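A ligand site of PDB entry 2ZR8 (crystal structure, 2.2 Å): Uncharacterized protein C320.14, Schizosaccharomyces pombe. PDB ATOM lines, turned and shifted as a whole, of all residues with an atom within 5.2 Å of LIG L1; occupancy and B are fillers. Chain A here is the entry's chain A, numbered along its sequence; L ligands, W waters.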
ATOM      1  N   ALA A  55     -17.994  27.099 -10.743  1.00  0.00           N
ATOM      2  CA  ALA A  55     -16.655  27.319 -11.273  1.00  0.00           C
ATOM      3  C   ALA A  55     -16.358  28.798 -11.364  1.00  0.00           C
ATOM      4  O   ALA A  55     -17.254  29.629 -11.255  1.00  0.00           O
ATOM      5  CB  ALA A  55     -16.500  26.665 -12.632  1.00  0.00           C
ATOM      6  N   PHE A  56     -15.095  29.114 -11.587  1.00  0.00           N
ATOM      7  CA  PHE A  56     -14.649  30.489 -11.691  1.00  0.00           C
ATOM      8  C   PHE A  56     -15.208  31.243 -12.900  1.00  0.00           C
ATOM      9  O   PHE A  56     -15.258  32.469 -12.888  1.00  0.00           O
ATOM     10  CB  PHE A  56     -13.116  30.520 -11.726  1.00  0.00           C
ATOM     11  CG  PHE A  56     -12.511  30.110 -13.054  1.00  0.00           C
ATOM     12  CD1 PHE A  56     -12.255  31.065 -14.043  1.00  0.00           C
ATOM     13  CD2 PHE A  56     -12.206  28.780 -13.308  1.00  0.00           C
ATOM     14  CE1 PHE A  56     -11.694  30.693 -15.271  1.00  0.00           C
ATOM     15  CE2 PHE A  56     -11.652  28.396 -14.533  1.00  0.00           C
ATOM     16  CZ  PHE A  56     -11.389  29.357 -15.512  1.00  0.00           C
ATOM     17  N   LYS A  57     -15.637  30.506 -13.918  1.00  0.00           N
ATOM     18  CA  LYS A  57     -16.158  31.105 -15.153  1.00  0.00           C
ATOM     19  C   LYS A  57     -17.244  32.169 -15.046  1.00  0.00           C
ATOM     20  O   LYS A  57     -17.385  32.998 -15.942  1.00  0.00           O
ATOM     21  CB  LYS A  57     -16.652  30.004 -16.092  1.00  0.00           C
ATOM     22  CG  LYS A  57     -15.544  29.150 -16.686  1.00  0.00           C
ATOM     23  CD  LYS A  57     -14.638  29.955 -17.624  1.00  0.00           C
ATOM     24  CE  LYS A  57     -13.577  29.044 -18.227  1.00  0.00           C
ATOM     25  NZ  LYS A  57     -13.243  29.264 -19.659  1.00  0.00           N
ATOM     26  N   PHE A  80     -18.854  29.106 -27.334  1.00  0.00           N
ATOM     27  CA  PHE A  80     -18.456  27.722 -27.450  1.00  0.00           C
ATOM     28  C   PHE A  80     -17.707  27.428 -26.157  1.00  0.00           C
ATOM     29  O   PHE A  80     -16.907  28.240 -25.706  1.00  0.00           O
ATOM     30  CB  PHE A  80     -17.558  27.506 -28.675  1.00  0.00           C
ATOM     31  CG  PHE A  80     -16.471  28.541 -28.844  1.00  0.00           C
ATOM     32  CD1 PHE A  80     -15.166  28.275 -28.459  1.00  0.00           C
ATOM     33  CD2 PHE A  80     -16.758  29.781 -29.446  1.00  0.00           C
ATOM     34  CE1 PHE A  80     -14.143  29.213 -28.668  1.00  0.00           C
ATOM     35  CE2 PHE A  80     -15.742  30.731 -29.658  1.00  0.00           C
ATOM     36  CZ  PHE A  80     -14.431  30.444 -29.275  1.00  0.00           C
ATOM     37  N   SER A  81     -17.974  26.268 -25.559  1.00  0.00           N
ATOM     38  CA  SER A  81     -17.355  25.951 -24.290  1.00  0.00           C
ATOM     39  C   SER A  81     -17.382  24.469 -23.933  1.00  0.00           C
ATOM     40  O   SER A  81     -18.275  23.734 -24.368  1.00  0.00           O
ATOM     41  CB  SER A  81     -18.082  26.746 -23.186  1.00  0.00           C
ATOM     42  OG  SER A  81     -17.847  26.196 -21.906  1.00  0.00           O
ATOM     43  N   SER A  82     -16.409  24.042 -23.148  1.00  0.00           N
ATOM     44  CA  SER A  82     -16.335  22.655 -22.698  1.00  0.00           C
ATOM     45  C   SER A  82     -17.377  22.390 -21.620  1.00  0.00           C
ATOM     46  O   SER A  82     -17.548  21.255 -21.180  1.00  0.00           O
ATOM     47  CB  SER A  82     -14.949  22.353 -22.137  1.00  0.00           C
ATOM     48  OG  SER A  82     -14.592  23.291 -21.143  1.00  0.00           O
ATOM     49  N   GLY A  83     -18.042  23.454 -21.176  1.00  0.00           N
ATOM     50  CA  GLY A  83     -19.088  23.276 -20.177  1.00  0.00           C
ATOM     51  C   GLY A  83     -19.245  24.325 -19.090  1.00  0.00           C
ATOM     52  O   GLY A  83     -20.365  24.712 -18.782  1.00  0.00           O
ATOM     53  N   ASN A  84     -18.153  24.783 -18.496  1.00  0.00           N
ATOM     54  CA  ASN A  84     -18.259  25.772 -17.434  1.00  0.00           C
ATOM     55  C   ASN A  84     -18.561  27.173 -17.923  1.00  0.00           C
ATOM     56  O   ASN A  84     -19.375  27.861 -17.330  1.00  0.00           O
ATOM     57  CB  ASN A  84     -17.009  25.720 -16.531  1.00  0.00           C
ATOM     58  CG  ASN A  84     -17.028  24.510 -15.602  1.00  0.00           C
ATOM     59  OD1 ASN A  84     -18.095  24.002 -15.268  1.00  0.00           O
ATOM     60  ND2 ASN A  84     -15.855  24.050 -15.167  1.00  0.00           N
ATOM     61  N   HIS A  85     -17.897  27.600 -19.003  1.00  0.00           N
ATOM     62  CA  HIS A  85     -18.170  28.929 -19.561  1.00  0.00           C
ATOM     63  C   HIS A  85     -19.614  28.889 -20.072  1.00  0.00           C
ATOM     64  O   HIS A  85     -20.331  29.870 -19.993  1.00  0.00           O
ATOM     65  CB  HIS A  85     -17.220  29.236 -20.721  1.00  0.00           C
ATOM     66  CG  HIS A  85     -17.361  30.626 -21.269  1.00  0.00           C
ATOM     67  ND1 HIS A  85     -17.210  31.754 -20.487  1.00  0.00           N
ATOM     68  CD2 HIS A  85     -17.610  31.069 -22.524  1.00  0.00           C
ATOM     69  CE1 HIS A  85     -17.351  32.829 -21.242  1.00  0.00           C
ATOM     70  NE2 HIS A  85     -17.592  32.440 -22.483  1.00  0.00           N
ATOM     71  N   ALA A  86     -20.007  27.729 -20.600  1.00  0.00           N
ATOM     72  CA  ALA A  86     -21.349  27.521 -21.120  1.00  0.00           C
ATOM     73  C   ALA A  86     -22.389  27.798 -20.039  1.00  0.00           C
ATOM     74  O   ALA A  86     -23.369  28.503 -20.265  1.00  0.00           O
ATOM     75  CB  ALA A  86     -21.491  26.096 -21.635  1.00  0.00           C
ATOM     76  N   LYS A 112     -22.918  19.426 -16.877  1.00  0.00           N
ATOM     77  CA  LYS A 112     -22.654  20.737 -17.443  1.00  0.00           C
ATOM     78  C   LYS A 112     -23.657  21.069 -18.544  1.00  0.00           C
ATOM     79  O   LYS A 112     -24.150  22.196 -18.626  1.00  0.00           O
ATOM     80  CB  LYS A 112     -21.219  20.802 -17.985  1.00  0.00           C
ATOM     81  CG  LYS A 112     -20.173  20.593 -16.902  1.00  0.00           C
ATOM     82  CD  LYS A 112     -18.773  20.855 -17.416  1.00  0.00           C
ATOM     83  CE  LYS A 112     -17.743  20.715 -16.312  1.00  0.00           C
ATOM     84  NZ  LYS A 112     -16.354  20.812 -16.817  1.00  0.00           N
ATOM     85  N   ARG A 133     -14.693  24.064 -33.524  1.00  0.00           N
ATOM     86  CA  ARG A 133     -15.726  24.834 -32.850  1.00  0.00           C
ATOM     87  C   ARG A 133     -15.701  26.337 -33.099  1.00  0.00           C
ATOM     88  O   ARG A 133     -16.749  26.988 -33.103  1.00  0.00           O
ATOM     89  CB  ARG A 133     -15.664  24.564 -31.347  1.00  0.00           C
ATOM     90  CG  ARG A 133     -14.423  25.076 -30.654  1.00  0.00           C
ATOM     91  CD  ARG A 133     -14.507  24.751 -29.174  1.00  0.00           C
ATOM     92  NE  ARG A 133     -13.402  25.336 -28.419  1.00  0.00           N
ATOM     93  CZ  ARG A 133     -13.365  25.403 -27.098  1.00  0.00           C
ATOM     94  NH1 ARG A 133     -14.368  24.924 -26.376  1.00  0.00           N
ATOM     95  NH2 ARG A 133     -12.316  25.960 -26.500  1.00  0.00           N
ATOM     96  N   PRO A 151     -14.697  31.770 -24.650  1.00  0.00           N
ATOM     97  CA  PRO A 151     -14.514  31.161 -23.325  1.00  0.00           C
ATOM     98  C   PRO A 151     -13.247  31.637 -22.602  1.00  0.00           C
ATOM     99  O   PRO A 151     -13.114  31.399 -21.399  1.00  0.00           O
ATOM    100  CB  PRO A 151     -14.491  29.674 -23.645  1.00  0.00           C
ATOM    101  CG  PRO A 151     -13.848  29.632 -25.003  1.00  0.00           C
ATOM    102  CD  PRO A 151     -14.564  30.769 -25.717  1.00  0.00           C
ATOM    103  N   TYR A 152     -12.338  32.286 -23.321  1.00  0.00           N
ATOM    104  CA  TYR A 152     -11.102  32.774 -22.700  1.00  0.00           C
ATOM    105  C   TYR A 152     -10.313  33.856 -23.446  1.00  0.00           C
ATOM    106  O   TYR A 152      -9.785  34.759 -22.819  1.00  0.00           O
ATOM    107  CB  TYR A 152     -10.166  31.604 -22.391  1.00  0.00           C
ATOM    108  CG  TYR A 152      -9.911  30.668 -23.561  1.00  0.00           C
ATOM    109  CD1 TYR A 152      -9.038  31.026 -24.593  1.00  0.00           C
ATOM    110  CD2 TYR A 152     -10.558  29.438 -23.635  1.00  0.00           C
ATOM    111  CE1 TYR A 152      -8.825  30.167 -25.678  1.00  0.00           C
ATOM    112  CE2 TYR A 152     -10.358  28.583 -24.702  1.00  0.00           C
ATOM    113  CZ  TYR A 152      -9.499  28.946 -25.717  1.00  0.00           C
ATOM    114  OH  TYR A 152      -9.320  28.090 -26.777  1.00  0.00           O
ATOM    115  N   CYS A 181      -4.746  26.545 -12.917  1.00  0.00           N
ATOM    116  CA  CYS A 181      -5.077  25.575 -13.939  1.00  0.00           C
ATOM    117  C   CYS A 181      -5.008  26.255 -15.303  1.00  0.00           C
ATOM    118  O   CYS A 181      -5.341  27.439 -15.423  1.00  0.00           O
ATOM    119  CB  CYS A 181      -6.476  25.013 -13.673  1.00  0.00           C
ATOM    120  SG  CYS A 181      -6.715  24.498 -11.941  1.00  0.00           S
ATOM    121  N   LEU A 182      -4.585  25.530 -16.333  1.00  0.00           N
ATOM    122  CA  LEU A 182      -4.456  26.135 -17.659  1.00  0.00           C
ATOM    123  C   LEU A 182      -5.102  25.402 -18.827  1.00  0.00           C
ATOM    124  O   LEU A 182      -4.715  24.279 -19.180  1.00  0.00           O
ATOM    125  CB  LEU A 182      -2.974  26.374 -17.975  1.00  0.00           C
ATOM    126  CG  LEU A 182      -2.667  26.919 -19.373  1.00  0.00           C
ATOM    127  CD1 LEU A 182      -3.279  28.302 -19.525  1.00  0.00           C
ATOM    128  CD2 LEU A 182      -1.159  26.977 -19.573  1.00  0.00           C
ATOM    129  N   GLY A 183      -6.081  26.071 -19.436  1.00  0.00           N
ATOM    130  CA  GLY A 183      -6.762  25.546 -20.602  1.00  0.00           C
ATOM    131  C   GLY A 183      -6.375  26.511 -21.718  1.00  0.00           C
ATOM    132  O   GLY A 183      -5.275  26.451 -22.235  1.00  0.00           O
ATOM    133  N   GLY A 184      -7.295  27.419 -22.052  1.00  0.00           N
ATOM    134  CA  GLY A 184      -7.031  28.410 -23.080  1.00  0.00           C
ATOM    135  C   GLY A 184      -6.177  29.555 -22.552  1.00  0.00           C
ATOM    136  O   GLY A 184      -5.575  30.309 -23.335  1.00  0.00           O
ATOM    137  N   GLY A 185      -6.126  29.718 -21.229  1.00  0.00           N
ATOM    138  CA  GLY A 185      -5.306  30.768 -20.649  1.00  0.00           C
ATOM    139  C   GLY A 185      -6.028  31.970 -20.056  1.00  0.00           C
ATOM    140  O   GLY A 185      -5.383  32.908 -19.591  1.00  0.00           O
ATOM    141  N   GLY A 186      -7.356  31.948 -20.055  1.00  0.00           N
ATOM    142  CA  GLY A 186      -8.106  33.066 -19.490  1.00  0.00           C
ATOM    143  C   GLY A 186      -7.889  33.187 -17.993  1.00  0.00           C
ATOM    144  O   GLY A 186      -7.607  34.273 -17.474  1.00  0.00           O
ATOM    145  N   LEU A 187      -8.015  32.074 -17.276  1.00  0.00           N
ATOM    146  CA  LEU A 187      -7.814  32.088 -15.831  1.00  0.00           C
ATOM    147  C   LEU A 187      -6.381  32.462 -15.471  1.00  0.00           C
ATOM    148  O   LEU A 187      -6.155  33.294 -14.590  1.00  0.00           O
ATOM    149  CB  LEU A 187      -8.146  30.707 -15.240  1.00  0.00           C
ATOM    150  CG  LEU A 187      -7.759  30.531 -13.767  1.00  0.00           C
ATOM    151  CD1 LEU A 187      -8.508  31.539 -12.911  1.00  0.00           C
ATOM    152  CD2 LEU A 187      -8.065  29.093 -13.330  1.00  0.00           C
ATOM    153  N   LEU A 188      -5.416  31.836 -16.139  1.00  0.00           N
ATOM    154  CA  LEU A 188      -4.012  32.121 -15.870  1.00  0.00           C
ATOM    155  C   LEU A 188      -3.632  33.566 -16.182  1.00  0.00           C
ATOM    156  O   LEU A 188      -3.008  34.241 -15.366  1.00  0.00           O
ATOM    157  CB  LEU A 188      -3.103  31.159 -16.661  1.00  0.00           C
ATOM    158  CG  LEU A 188      -1.589  31.335 -16.491  1.00  0.00           C
ATOM    159  CD1 LEU A 188      -1.172  31.089 -15.040  1.00  0.00           C
ATOM    160  CD2 LEU A 188      -0.855  30.355 -17.413  1.00  0.00           C
ATOM    161  N   GLY A 236     -11.763  20.220 -18.878  1.00  0.00           N
ATOM    162  CA  GLY A 236     -11.802  21.666 -19.005  1.00  0.00           C
ATOM    163  C   GLY A 236     -10.494  22.252 -19.522  1.00  0.00           C
ATOM    164  O   GLY A 236     -10.357  23.467 -19.599  1.00  0.00           O
ATOM    165  N   THR A 239      -8.007  22.208 -24.636  1.00  0.00           N
ATOM    166  CA  THR A 239      -7.822  23.195 -25.689  1.00  0.00           C
ATOM    167  C   THR A 239      -6.659  22.763 -26.575  1.00  0.00           C
ATOM    168  O   THR A 239      -5.709  22.141 -26.100  1.00  0.00           O
ATOM    169  CB  THR A 239      -7.524  24.581 -25.083  1.00  0.00           C
ATOM    170  OG1 THR A 239      -6.803  24.422 -23.849  1.00  0.00           O
ATOM    171  CG2 THR A 239      -8.797  25.347 -24.824  1.00  0.00           C
ATOM    172  N   GLU A 281     -13.515  19.026  -9.593  1.00  0.00           N
ATOM    173  CA  GLU A 281     -13.489  18.316 -10.869  1.00  0.00           C
ATOM    174  C   GLU A 281     -12.025  18.111 -11.262  1.00  0.00           C
ATOM    175  O   GLU A 281     -11.152  18.879 -10.853  1.00  0.00           O
ATOM    176  CB  GLU A 281     -14.271  19.069 -11.955  1.00  0.00           C
ATOM    177  CG  GLU A 281     -13.883  20.500 -12.235  1.00  0.00           C
ATOM    178  CD  GLU A 281     -14.728  21.073 -13.343  1.00  0.00           C
ATOM    179  OE1 GLU A 281     -14.582  20.622 -14.510  1.00  0.00           O
ATOM    180  OE2 GLU A 281     -15.544  21.979 -13.065  1.00  0.00           O
ATOM    181  N   THR A 283     -10.158  18.828 -13.747  1.00  0.00           N
ATOM    182  CA  THR A 283      -9.453  20.005 -14.209  1.00  0.00           C
ATOM    183  C   THR A 283      -9.092  20.923 -13.039  1.00  0.00           C
ATOM    184  O   THR A 283      -8.061  21.597 -13.060  1.00  0.00           O
ATOM    185  CB  THR A 283     -10.283  20.772 -15.267  1.00  0.00           C
ATOM    186  OG1 THR A 283     -10.674  19.865 -16.301  1.00  0.00           O
ATOM    187  CG2 THR A 283      -9.466  21.895 -15.882  1.00  0.00           C
ATOM    188  N   GLY A 284      -9.939  20.947 -12.017  1.00  0.00           N
ATOM    189  CA  GLY A 284      -9.676  21.781 -10.860  1.00  0.00           C
ATOM    190  C   GLY A 284      -8.560  21.237  -9.977  1.00  0.00           C
ATOM    191  O   GLY A 284      -8.131  21.910  -9.040  1.00  0.00           O
ATOM    192  N   SER A 308     -10.284  25.808  -9.377  1.00  0.00           N
ATOM    193  CA  SER A 308     -11.124  26.337 -10.435  1.00  0.00           C
ATOM    194  C   SER A 308     -12.575  25.889 -10.511  1.00  0.00           C
ATOM    195  O   SER A 308     -13.432  26.680 -10.863  1.00  0.00           O
ATOM    196  CB  SER A 308     -10.449  26.123 -11.804  1.00  0.00           C
ATOM    197  OG  SER A 308     -10.290  24.732 -12.068  1.00  0.00           O
ATOM    198  N   GLY A 309     -12.864  24.639 -10.188  1.00  0.00           N
ATOM    199  CA  GLY A 309     -14.237  24.197 -10.269  1.00  0.00           C
ATOM    200  C   GLY A 309     -14.551  22.857  -9.647  1.00  0.00           C
ATOM    201  O   GLY A 309     -13.649  22.105  -9.294  1.00  0.00           O
HETATM  202  N1  LIG L   1     -13.011  26.401 -19.058  1.00  0.00           N
HETATM  203  N2  LIG L   1     -10.682  24.770 -14.540  1.00  0.00           N
HETATM  204  C1  LIG L   1     -12.025  24.448 -14.863  1.00  0.00           C
HETATM  205  C2  LIG L   1     -12.890  23.793 -13.847  1.00  0.00           C
HETATM  206  C3  LIG L   1     -12.524  24.801 -16.216  1.00  0.00           C
HETATM  207  O1  LIG L   1     -13.773  24.583 -16.702  1.00  0.00           O
HETATM  208  C4  LIG L   1     -11.527  25.481 -17.160  1.00  0.00           C
HETATM  209  C5  LIG L   1     -11.910  25.890 -18.567  1.00  0.00           C
HETATM  210  C6  LIG L   1     -10.176  25.762 -16.740  1.00  0.00           C
HETATM  211  C7  LIG L   1      -9.158  26.442 -17.661  1.00  0.00           C
HETATM  212  O2  LIG L   1      -9.393  27.819 -18.030  1.00  0.00           O
HETATM  213  P1  LIG L   1      -8.780  28.466 -19.133  1.00  0.00           P
HETATM  214  O3  LIG L   1      -9.360  27.767 -20.342  1.00  0.00           O
HETATM  215  O4  LIG L   1      -9.261  29.812 -19.117  1.00  0.00           O
HETATM  216  O5  LIG L   1      -7.418  28.497 -19.421  1.00  0.00           O
HETATM  217  C8  LIG L   1      -9.757  25.384 -15.389  1.00  0.00           C
HETATM  218  C9  LIG L   1     -13.358  26.808 -20.442  1.00  0.00           C
HETATM  219  C10 LIG L   1     -13.135  28.280 -20.658  1.00  0.00           C
HETATM  220  C11 LIG L   1     -14.897  26.522 -20.734  1.00  0.00           C
HETATM  221  O6  LIG L   1     -15.627  26.041 -19.876  1.00  0.00           O
HETATM  222  O7  LIG L   1     -15.402  26.775 -21.846  1.00  0.00           O
HETATM  223  N1  LG2 L   2     -10.848  25.085 -21.935  1.00  0.00           N
HETATM  224  C1  LG2 L   2     -11.441  24.223 -22.959  1.00  0.00           C
HETATM  225  C2  LG2 L   2     -12.720  24.789 -23.602  1.00  0.00           C
HETATM  226  O1  LG2 L   2     -12.955  26.031 -23.644  1.00  0.00           O
HETATM  227  C3  LG2 L   2     -11.785  22.870 -22.326  1.00  0.00           C
HETATM  228  O2  LG2 L   2     -11.192  21.792 -23.012  1.00  0.00           O
HETATM  229  O3  LG2 L   2     -13.565  24.062 -24.117  1.00  0.00           O
HETATM  230  O   HOH W   1      -5.819  29.451 -17.481  1.00  0.00           O
HETATM  231  O   HOH W   2     -15.349  23.054 -18.438  1.00  0.00           O
HETATM  232  O   HOH W   3     -11.336  31.770 -19.242  1.00  0.00           O
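O3 of LIG L1 lies within hydrogen-bond range of N of Gly 184 (2.7 Å). O3 of LG2 L2 lies close to OG of Ser 82 (3.2 Å). O7 of LIG L1 is in hydrogen-bond range of N of Ser 82 (3.2 Å). O4 of LIG L1 is in hydrogen-bond range of N of Leu 187 (3.2 Å). The side-chain hydroxyl (OG) of Ser 82 sits at hydrogen-bond distance from an oxygen (O6) of LIG L1 (3.2 Å). The side-chain amino group (NZ) of Lys 57 is bonded to a carbon (C10) of LIG L1, 1.4 Å away. N of His 85 is in hydrogen-bond range of O6 of LIG L1 (2.9 Å). The backbone carbonyl oxygen (O) of Gly 236 sits at hydrogen-bond distance from a nitrogen (N1) of LG2 L2 (2.9 Å). N2 of LIG L1 sits at hydrogen-bond distance from OG of Ser 308 (2.5 Å). O3 of LG2 L2 lies close to N of Ser 82 (3.0 Å). The side-chain hydroxyl (OG) of Ser 81 lies within hydrogen-bond range of an oxygen (O7) of LIG L1. O3 of LG2 L2 is in salt-bridge range of NH1 of Arg 133 (2.5 Å). The backbone NH (N) of Gly 185 is in hydrogen-bond range of an oxygen (O5) of LIG L1. ND2 of Asn 84 sits at hydrogen-bond distance from O1 of LIG L1 (2.6 Å). The backbone NH of Gly 186 lies within hydrogen-bond range of an oxygen (O4) of LIG L1 (3.0 Å). The backbone NH (N) of Gly 183 sits at hydrogen-bond distance from an oxygen (O5) of LIG L1 (2.8 Å). The backbone NH (N) of Asn 84 is in hydrogen-bond range of an oxygen (O6) of LIG L1, at 3.1 Å.
An oxygen (O3) of LIG L1 sits close to a nitrogen (N1) of LG2 L2, 3.5 Å away.
N of Ala 86 sits at hydrogen-bond distance from OG of Ser 81. O of Gly 183 sits at hydrogen-bond distance from OG1 of Thr 239. The backbone NH (N) of Glu 281 sits at hydrogen-bond distance from the backbone carbonyl oxygen (O) of Gly 309. The side-chain carboxylate (OE1) of Glu 281 is in salt-bridge range of the side-chain amino group (NZ) of Lys 112, at 2.9 Å. The side-chain hydroxyl of Ser 81 is in hydrogen-bond range of the backbone NH of Gly 83, at 2.8 Å. OG1 of Thr 283 lies within hydrogen-bond range of N of Gly 236 (2.8 Å). ND2 of Asn 84 sits at hydrogen-bond distance from OE2 of Glu 281 (3.0 Å). OG of Ser 308 is in hydrogen-bond range of SG of Cys 181, at 3.6 Å.
CZ of Phe 56 touches O2 of LIG L1, 3.6 Å away. Gly 83 touches LIG L1. Pro 151 touches LIG L1 (O to C10, 3.2 Å). Tyr 152 touches LIG L1. Cys 181 touches LIG L1. Leu 182 touches LIG L1 (C to O5, 3.9 Å). Gly 236 touches LIG L1. Glu 281 touches LIG L1 (OE2 to C2, 3.3 Å). CG2 of Thr 283 touches N2 of LIG L1, 3.4 Å away. Gly 309 touches LIG L1. Hydrophobic or aromatic side chains that line LIG L1: Phe 56, His 85, Pro 151 and Tyr 152. 21 residues have an atom within 4 Å of LIG L1: Phe 56, Lys 57, Ser 81, Ser 82, Gly 83, Asn 84, His 85, Pro 151, Tyr 152, Cys 181, Leu 182, Gly 183, Gly 184, Gly 185, Gly 186, Leu 187, Gly 236, Glu 281, Thr 283, Ser 308 and Gly 309. The nearest printed residue that does not touch LIG L1 is Phe 80 (4.4 Å).
Water W1 lies within hydrogen-bond range of an oxygen (O5) of LIG L1 (2.7 Å), the backbone NH of Leu 188 (2.8 Å), the backbone carbonyl oxygen of Cys 181 (2.9 Å) and the backbone NH of Leu 187 (3.4 Å). Water W2 lies within hydrogen-bond range of an oxygen (O1) of LIG L1 (2.8 Å), the side-chain hydroxyl of Ser 82 (2.8 Å), the side-chain amino group of Lys 112 (2.9 Å) and the backbone NH of Asn 84 (3.3 Å). Water W3 lies within hydrogen-bond range of the backbone carbonyl oxygen of Pro 151 (2.8 Å), an oxygen (O4) of LIG L1 (2.9 Å) and the side-chain amino group of Lys 57 (3.2 Å).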
